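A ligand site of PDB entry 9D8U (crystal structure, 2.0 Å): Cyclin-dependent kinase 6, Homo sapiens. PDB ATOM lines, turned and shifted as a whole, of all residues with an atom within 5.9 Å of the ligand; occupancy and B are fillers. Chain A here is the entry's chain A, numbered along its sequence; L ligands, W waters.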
ATOM      1  N   ILE A  19     -30.123   2.571  19.568  1.00  0.00           N
ATOM      2  CA  ILE A  19     -29.534   2.798  20.890  1.00  0.00           C
ATOM      3  C   ILE A  19     -30.533   2.343  21.985  1.00  0.00           C
ATOM      4  O   ILE A  19     -30.144   1.723  22.971  1.00  0.00           O
ATOM      5  CB  ILE A  19     -29.106   4.283  21.033  1.00  0.00           C
ATOM      6  CG1 ILE A  19     -27.876   4.594  20.167  1.00  0.00           C
ATOM      7  CG2 ILE A  19     -28.858   4.662  22.481  1.00  0.00           C
ATOM      8  CD1 ILE A  19     -27.471   6.095  20.154  1.00  0.00           C
ATOM      9  N   GLY A  20     -31.818   2.625  21.774  1.00  0.00           N
ATOM     10  CA  GLY A  20     -32.852   2.238  22.718  1.00  0.00           C
ATOM     11  C   GLY A  20     -34.258   2.587  22.285  1.00  0.00           C
ATOM     12  O   GLY A  20     -34.517   3.060  21.168  1.00  0.00           O
ATOM     13  N   GLU A  21     -35.218   2.309  23.182  1.00  0.00           N
ATOM     14  CA  GLU A  21     -36.637   2.636  22.900  1.00  0.00           C
ATOM     15  C   GLU A  21     -37.219   3.443  24.062  1.00  0.00           C
ATOM     16  O   GLU A  21     -36.990   3.044  25.220  1.00  0.00           O
ATOM     17  CB  GLU A  21     -37.457   1.365  22.642  1.00  0.00           C
ATOM     18  CG  GLU A  21     -37.191   0.745  21.290  1.00  0.00           C
ATOM     19  CD  GLU A  21     -38.104  -0.419  20.945  1.00  0.00           C
ATOM     20  OE1 GLU A  21     -39.331  -0.220  20.919  1.00  0.00           O
ATOM     21  OE2 GLU A  21     -37.581  -1.520  20.696  1.00  0.00           O
ATOM     22  N   GLY A  22     -37.937   4.523  23.754  1.00  0.00           N
ATOM     23  CA  GLY A  22     -38.576   5.338  24.810  1.00  0.00           C
ATOM     24  C   GLY A  22     -40.058   5.496  24.556  1.00  0.00           C
ATOM     25  O   GLY A  22     -40.528   5.025  23.500  1.00  0.00           O
ATOM     26  N   ALA A  23     -40.782   6.099  25.492  1.00  0.00           N
ATOM     27  CA  ALA A  23     -42.224   6.373  25.292  1.00  0.00           C
ATOM     28  C   ALA A  23     -42.377   7.514  24.284  1.00  0.00           C
ATOM     29  O   ALA A  23     -41.541   8.437  24.302  1.00  0.00           O
ATOM     30  CB  ALA A  23     -42.871   6.706  26.604  1.00  0.00           C
ATOM     31  N   VAL A  27     -34.532   5.571  19.758  1.00  0.00           N
ATOM     32  CA  VAL A  27     -33.308   6.358  19.804  1.00  0.00           C
ATOM     33  C   VAL A  27     -32.359   5.646  18.845  1.00  0.00           C
ATOM     34  O   VAL A  27     -32.209   4.428  18.933  1.00  0.00           O
ATOM     35  CB  VAL A  27     -32.711   6.428  21.232  1.00  0.00           C
ATOM     36  CG1 VAL A  27     -31.523   7.379  21.259  1.00  0.00           C
ATOM     37  CG2 VAL A  27     -33.768   6.871  22.230  1.00  0.00           C
ATOM     38  N   LYS A  29     -28.397   5.616  16.711  1.00  0.00           N
ATOM     39  CA  LYS A  29     -27.052   6.216  16.476  1.00  0.00           C
ATOM     40  C   LYS A  29     -27.036   6.598  14.995  1.00  0.00           C
ATOM     41  O   LYS A  29     -27.282   5.714  14.160  1.00  0.00           O
ATOM     42  CB  LYS A  29     -25.939   5.216  16.818  1.00  0.00           C
ATOM     43  CG  LYS A  29     -24.521   5.713  16.608  1.00  0.00           C
ATOM     44  CD  LYS A  29     -23.477   4.687  16.988  1.00  0.00           C
ATOM     45  CE  LYS A  29     -22.064   5.194  16.874  1.00  0.00           C
ATOM     46  NZ  LYS A  29     -21.075   4.161  17.264  1.00  0.00           N
ATOM     47  N   ALA A  41     -26.856  11.127  18.332  1.00  0.00           N
ATOM     48  CA  ALA A  41     -27.968  10.320  18.880  1.00  0.00           C
ATOM     49  C   ALA A  41     -29.289  10.988  18.470  1.00  0.00           C
ATOM     50  O   ALA A  41     -29.533  12.117  18.914  1.00  0.00           O
ATOM     51  CB  ALA A  41     -27.839  10.216  20.373  1.00  0.00           C
ATOM     52  N   LYS A  43     -33.295  11.177  18.587  1.00  0.00           N
ATOM     53  CA  LYS A  43     -34.497  10.730  19.330  1.00  0.00           C
ATOM     54  C   LYS A  43     -35.735  11.335  18.670  1.00  0.00           C
ATOM     55  O   LYS A  43     -35.782  12.569  18.520  1.00  0.00           O
ATOM     56  CB  LYS A  43     -34.413  11.144  20.810  1.00  0.00           C
ATOM     57  CG  LYS A  43     -35.724  11.058  21.572  1.00  0.00           C
ATOM     58  CD  LYS A  43     -35.568  11.236  23.063  1.00  0.00           C
ATOM     59  CE  LYS A  43     -34.921  10.040  23.740  1.00  0.00           C
ATOM     60  NZ  LYS A  43     -34.863  10.205  25.204  1.00  0.00           N
ATOM     61  N   VAL A  77     -25.149  16.632  27.989  1.00  0.00           N
ATOM     62  CA  VAL A  77     -24.999  16.265  26.554  1.00  0.00           C
ATOM     63  C   VAL A  77     -25.427  17.464  25.693  1.00  0.00           C
ATOM     64  O   VAL A  77     -26.394  18.147  26.070  1.00  0.00           O
ATOM     65  CB  VAL A  77     -25.791  14.988  26.208  1.00  0.00           C
ATOM     66  CG1 VAL A  77     -27.285  15.184  26.378  1.00  0.00           C
ATOM     67  CG2 VAL A  77     -25.475  14.485  24.808  1.00  0.00           C
ATOM     68  N   PHE A  98     -28.577  14.916  19.290  1.00  0.00           N
ATOM     69  CA  PHE A  98     -27.654  15.151  20.425  1.00  0.00           C
ATOM     70  C   PHE A  98     -26.252  14.669  20.058  1.00  0.00           C
ATOM     71  O   PHE A  98     -26.126  13.881  19.101  1.00  0.00           O
ATOM     72  CB  PHE A  98     -28.108  14.364  21.646  1.00  0.00           C
ATOM     73  CG  PHE A  98     -29.392  14.823  22.290  1.00  0.00           C
ATOM     74  CD1 PHE A  98     -29.439  15.988  23.040  1.00  0.00           C
ATOM     75  CD2 PHE A  98     -30.552  14.081  22.149  1.00  0.00           C
ATOM     76  CE1 PHE A  98     -30.617  16.401  23.637  1.00  0.00           C
ATOM     77  CE2 PHE A  98     -31.740  14.504  22.742  1.00  0.00           C
ATOM     78  CZ  PHE A  98     -31.766  15.664  23.485  1.00  0.00           C
ATOM     79  N   GLU A  99     -25.238  15.106  20.791  1.00  0.00           N
ATOM     80  CA  GLU A  99     -23.883  14.579  20.572  1.00  0.00           C
ATOM     81  C   GLU A  99     -23.888  13.102  20.961  1.00  0.00           C
ATOM     82  O   GLU A  99     -24.601  12.748  21.900  1.00  0.00           O
ATOM     83  CB  GLU A  99     -22.836  15.358  21.374  1.00  0.00           C
ATOM     84  CG  GLU A  99     -22.908  15.166  22.863  1.00  0.00           C
ATOM     85  CD  GLU A  99     -21.813  15.864  23.639  1.00  0.00           C
ATOM     86  OE1 GLU A  99     -22.140  16.660  24.535  1.00  0.00           O
ATOM     87  OE2 GLU A  99     -20.632  15.614  23.350  1.00  0.00           O
ATOM     88  N   HIS A 100     -23.126  12.285  20.256  1.00  0.00           N
ATOM     89  CA  HIS A 100     -23.025  10.854  20.619  1.00  0.00           C
ATOM     90  C   HIS A 100     -21.848  10.642  21.571  1.00  0.00           C
ATOM     91  O   HIS A 100     -20.752  11.135  21.301  1.00  0.00           O
ATOM     92  CB  HIS A 100     -22.917   9.985  19.360  1.00  0.00           C
ATOM     93  CG  HIS A 100     -22.804   8.532  19.654  1.00  0.00           C
ATOM     94  ND1 HIS A 100     -21.636   7.937  20.065  1.00  0.00           N
ATOM     95  CD2 HIS A 100     -23.702   7.555  19.581  1.00  0.00           C
ATOM     96  CE1 HIS A 100     -21.839   6.655  20.240  1.00  0.00           C
ATOM     97  NE2 HIS A 100     -23.094   6.399  19.949  1.00  0.00           N
ATOM     98  N   VAL A 101     -22.089   9.946  22.671  1.00  0.00           N
ATOM     99  CA  VAL A 101     -21.005   9.559  23.611  1.00  0.00           C
ATOM    100  C   VAL A 101     -20.964   8.032  23.551  1.00  0.00           C
ATOM    101  O   VAL A 101     -22.028   7.417  23.613  1.00  0.00           O
ATOM    102  CB  VAL A 101     -21.194  10.119  25.030  1.00  0.00           C
ATOM    103  CG1 VAL A 101     -20.099   9.652  25.976  1.00  0.00           C
ATOM    104  CG2 VAL A 101     -21.315  11.637  25.037  1.00  0.00           C
ATOM    105  N   ASP A 102     -19.778   7.465  23.410  1.00  0.00           N
ATOM    106  CA  ASP A 102     -19.644   5.999  23.188  1.00  0.00           C
ATOM    107  C   ASP A 102     -20.095   5.157  24.394  1.00  0.00           C
ATOM    108  O   ASP A 102     -20.637   4.081  24.148  1.00  0.00           O
ATOM    109  CB  ASP A 102     -18.208   5.663  22.777  1.00  0.00           C
ATOM    110  CG  ASP A 102     -17.862   6.055  21.359  1.00  0.00           C
ATOM    111  OD1 ASP A 102     -18.629   5.705  20.450  1.00  0.00           O
ATOM    112  OD2 ASP A 102     -16.793   6.666  21.170  1.00  0.00           O
ATOM    113  N   GLN A 103     -19.861   5.616  25.613  1.00  0.00           N
ATOM    114  CA  GLN A 103     -20.165   4.731  26.766  1.00  0.00           C
ATOM    115  C   GLN A 103     -20.972   5.398  27.884  1.00  0.00           C
ATOM    116  O   GLN A 103     -20.921   6.614  28.017  1.00  0.00           O
ATOM    117  CB  GLN A 103     -18.861   4.129  27.321  1.00  0.00           C
ATOM    118  CG  GLN A 103     -18.131   4.958  28.354  1.00  0.00           C
ATOM    119  CD  GLN A 103     -16.768   4.370  28.610  1.00  0.00           C
ATOM    120  OE1 GLN A 103     -16.631   3.211  28.975  1.00  0.00           O
ATOM    121  NE2 GLN A 103     -15.739   5.177  28.396  1.00  0.00           N
ATOM    122  N   ASP A 104     -21.679   4.576  28.656  1.00  0.00           N
ATOM    123  CA  ASP A 104     -22.443   5.035  29.839  1.00  0.00           C
ATOM    124  C   ASP A 104     -21.628   4.613  31.061  1.00  0.00           C
ATOM    125  O   ASP A 104     -20.630   3.925  30.887  1.00  0.00           O
ATOM    126  CB  ASP A 104     -23.856   4.465  29.801  1.00  0.00           C
ATOM    127  CG  ASP A 104     -23.962   2.952  29.738  1.00  0.00           C
ATOM    128  OD1 ASP A 104     -22.950   2.284  29.961  1.00  0.00           O
ATOM    129  OD2 ASP A 104     -25.058   2.467  29.428  1.00  0.00           O
ATOM    130  N   THR A 107     -21.302   0.627  31.396  1.00  0.00           N
ATOM    131  CA  THR A 107     -20.286  -0.037  30.555  1.00  0.00           C
ATOM    132  C   THR A 107     -18.893   0.318  31.061  1.00  0.00           C
ATOM    133  O   THR A 107     -17.989  -0.520  30.954  1.00  0.00           O
ATOM    134  CB  THR A 107     -20.492   0.318  29.069  1.00  0.00           C
ATOM    135  OG1 THR A 107     -20.487   1.732  28.955  1.00  0.00           O
ATOM    136  CG2 THR A 107     -21.778  -0.238  28.515  1.00  0.00           C
ATOM    137  N   LYS A 147     -29.711   7.396  36.358  1.00  0.00           N
ATOM    138  CA  LYS A 147     -29.177   6.024  36.511  1.00  0.00           C
ATOM    139  C   LYS A 147     -27.899   5.892  35.680  1.00  0.00           C
ATOM    140  O   LYS A 147     -27.757   6.650  34.710  1.00  0.00           O
ATOM    141  CB  LYS A 147     -30.239   5.000  36.108  1.00  0.00           C
ATOM    142  CG  LYS A 147     -30.791   5.148  34.700  1.00  0.00           C
ATOM    143  CD  LYS A 147     -32.068   4.365  34.489  1.00  0.00           C
ATOM    144  CE  LYS A 147     -32.694   4.599  33.126  1.00  0.00           C
ATOM    145  NZ  LYS A 147     -33.963   3.852  32.974  1.00  0.00           N
ATOM    146  N   GLN A 149     -27.078   4.293  33.352  1.00  0.00           N
ATOM    147  CA  GLN A 149     -27.353   4.094  31.902  1.00  0.00           C
ATOM    148  C   GLN A 149     -27.517   5.442  31.191  1.00  0.00           C
ATOM    149  O   GLN A 149     -27.233   5.483  29.976  1.00  0.00           O
ATOM    150  CB  GLN A 149     -28.593   3.214  31.718  1.00  0.00           C
ATOM    151  CG  GLN A 149     -28.428   1.798  32.240  1.00  0.00           C
ATOM    152  CD  GLN A 149     -28.474   1.717  33.740  1.00  0.00           C
ATOM    153  OE1 GLN A 149     -27.523   1.271  34.393  1.00  0.00           O
ATOM    154  NE2 GLN A 149     -29.579   2.149  34.318  1.00  0.00           N
ATOM    155  N   ASN A 150     -27.963   6.476  31.897  1.00  0.00           N
ATOM    156  CA  ASN A 150     -28.181   7.814  31.273  1.00  0.00           C
ATOM    157  C   ASN A 150     -27.023   8.743  31.634  1.00  0.00           C
ATOM    158  O   ASN A 150     -26.993   9.873  31.138  1.00  0.00           O
ATOM    159  CB  ASN A 150     -29.539   8.408  31.636  1.00  0.00           C
ATOM    160  CG  ASN A 150     -29.811   8.446  33.119  1.00  0.00           C
ATOM    161  OD1 ASN A 150     -29.020   9.000  33.890  1.00  0.00           O
ATOM    162  ND2 ASN A 150     -30.922   7.864  33.533  1.00  0.00           N
ATOM    163  N   LEU A 152     -23.463   9.541  30.866  1.00  0.00           N
ATOM    164  CA  LEU A 152     -22.534   9.141  29.784  1.00  0.00           C
ATOM    165  C   LEU A 152     -21.100   9.541  30.110  1.00  0.00           C
ATOM    166  O   LEU A 152     -20.903  10.608  30.713  1.00  0.00           O
ATOM    167  CB  LEU A 152     -23.033   9.759  28.474  1.00  0.00           C
ATOM    168  CG  LEU A 152     -24.479   9.417  28.121  1.00  0.00           C
ATOM    169  CD1 LEU A 152     -24.847   9.916  26.738  1.00  0.00           C
ATOM    170  CD2 LEU A 152     -24.721   7.922  28.232  1.00  0.00           C
ATOM    171  N   ALA A 162     -27.604  12.847  30.145  1.00  0.00           N
ATOM    172  CA  ALA A 162     -28.444  12.621  28.994  1.00  0.00           C
ATOM    173  C   ALA A 162     -29.821  12.079  29.477  1.00  0.00           C
ATOM    174  O   ALA A 162     -29.974  11.713  30.660  1.00  0.00           O
ATOM    175  CB  ALA A 162     -27.779  11.578  28.098  1.00  0.00           C
ATOM    176  N   ASP A 163     -30.823  12.065  28.550  1.00  0.00           N
ATOM    177  CA  ASP A 163     -32.129  11.452  28.749  1.00  0.00           C
ATOM    178  C   ASP A 163     -32.945  12.083  29.876  1.00  0.00           C
ATOM    179  O   ASP A 163     -33.396  11.393  30.781  1.00  0.00           O
ATOM    180  CB  ASP A 163     -31.935   9.945  28.943  1.00  0.00           C
ATOM    181  CG  ASP A 163     -33.199   9.127  28.825  1.00  0.00           C
ATOM    182  OD1 ASP A 163     -34.160   9.615  28.217  1.00  0.00           O
ATOM    183  OD2 ASP A 163     -33.212   7.985  29.368  1.00  0.00           O
HETATM  184  C1  LIG L   1     -29.332   7.883  25.224  1.00  0.00           C
HETATM  185  C2  LIG L   1     -29.867   9.870  23.980  1.00  0.00           C
HETATM  186  C3  LIG L   1     -25.569  10.387  23.474  1.00  0.00           C
HETATM  187  C4  LIG L   1     -28.913   8.973  24.462  1.00  0.00           C
HETATM  188  C5  LIG L   1     -31.652   8.600  24.993  1.00  0.00           C
HETATM  189  C6  LIG L   1     -30.686   7.722  25.470  1.00  0.00           C
HETATM  190  C7  LIG L   1     -31.202   9.679  24.275  1.00  0.00           C
HETATM  191  C8  LIG L   1     -26.874  10.382  23.924  1.00  0.00           C
HETATM  192  C9  LIG L   1     -27.469   9.148  24.158  1.00  0.00           C
HETATM  193  C10 LIG L   1     -32.734   7.017  25.947  1.00  0.00           C
HETATM  194  C11 LIG L   1     -25.510   8.123  23.583  1.00  0.00           C
HETATM  195  C12 LIG L   1     -25.133   5.417  25.268  1.00  0.00           C
HETATM  196  C13 LIG L   1     -25.445   3.970  25.575  1.00  0.00           C
HETATM  197  C14 LIG L   1     -24.868   3.219  23.406  1.00  0.00           C
HETATM  198  C15 LIG L   1     -25.228   5.647  23.757  1.00  0.00           C
HETATM  199  C16 LIG L   1     -24.410   4.608  22.994  1.00  0.00           C
HETATM  200  C17 LIG L   1     -29.930   6.080  27.996  1.00  0.00           C
HETATM  201  C18 LIG L   1     -30.070   4.613  25.941  1.00  0.00           C
HETATM  202  C19 LIG L   1     -33.914   4.821  25.737  1.00  0.00           C
HETATM  203  C20 LIG L   1     -35.287   6.849  26.279  1.00  0.00           C
HETATM  204  C21 LIG L   1     -30.801   5.574  26.861  1.00  0.00           C
HETATM  205  C22 LIG L   1     -33.924   6.172  26.439  1.00  0.00           C
HETATM  206  N1  LIG L   1     -24.864   9.265  23.296  1.00  0.00           N
HETATM  207  N2  LIG L   1     -32.927   8.141  25.298  1.00  0.00           N
HETATM  208  N3  LIG L   1     -26.784   8.007  24.020  1.00  0.00           N
HETATM  209  N4  LIG L   1     -31.406   6.708  26.101  1.00  0.00           N
HETATM  210  N5  LIG L   1     -24.807   6.992  23.390  1.00  0.00           N
HETATM  211  O1  LIG L   1     -24.619   3.076  24.820  1.00  0.00           O
HETATM  212  O2  LIG L   1     -24.535   4.758  21.588  1.00  0.00           O
HETATM  213  O3  LIG L   1     -33.775   5.930  27.843  1.00  0.00           O
HETATM  214  F1  LIG L   1     -32.097  10.608  23.895  1.00  0.00           F
HETATM  215 CL1  LIG L   1     -27.642  11.893  24.304  1.00  0.00          CL
HETATM  216  O   HOH W   1     -25.180   0.040  26.207  1.00  0.00           O
HETATM  217  O   HOH W   2     -27.726   3.141  28.081  1.00  0.00           O
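The backbone carbonyl oxygen of Phe 98 sits at hydrogen-bond distance from the backbone NH of Ala 41, 3.0 Å away.
N of Ile 19 sits at hydrogen-bond distance from O of Val 27 (2.9 Å).
The side-chain carboxylate (OD1) of Asp 163 lies within salt-bridge range of the side-chain amino group (NZ) of Lys 43 (3.1 Å).
O of Gly 20 lies within hydrogen-bond range of N of Val 27 (2.9 Å).
The backbone carbonyl oxygen (O) of Asn 150 sits at hydrogen-bond distance from the backbone NH (N) of Ala 162 (3.2 Å).
Water W2 lies within hydrogen-bond range of the backbone carbonyl oxygen of Gln 149 (3.1 Å) and the side-chain carboxylate of Asp 104 (3.1 Å).
Residues that only touch the ligand: Glu 99, Leu 152, Gln 149, Val 77, Val 27, Ile 19, Glu 21, Phe 98, Ala 41, Ala 162, Gly 22 and Asp 102.
The nearest printed residue that does not touch the ligand is Asn 150 (4.1 Å).
N of Val 101 lies within hydrogen-bond range of N1 of the ligand (2.9 Å).
N2 of the ligand is in hydrogen-bond range of NZ of Lys 43.
A ring nitrogen (NE2) of His 100 is in hydrogen-bond range of an oxygen (O2) of the ligand, at 2.7 Å.
The backbone carbonyl oxygen (O) of Val 101 lies within hydrogen-bond range of a nitrogen (N5) of the ligand.
The side-chain carboxylate (OD2) of Asp 163 sits at hydrogen-bond distance from an oxygen (O3) of the ligand (2.6 Å).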
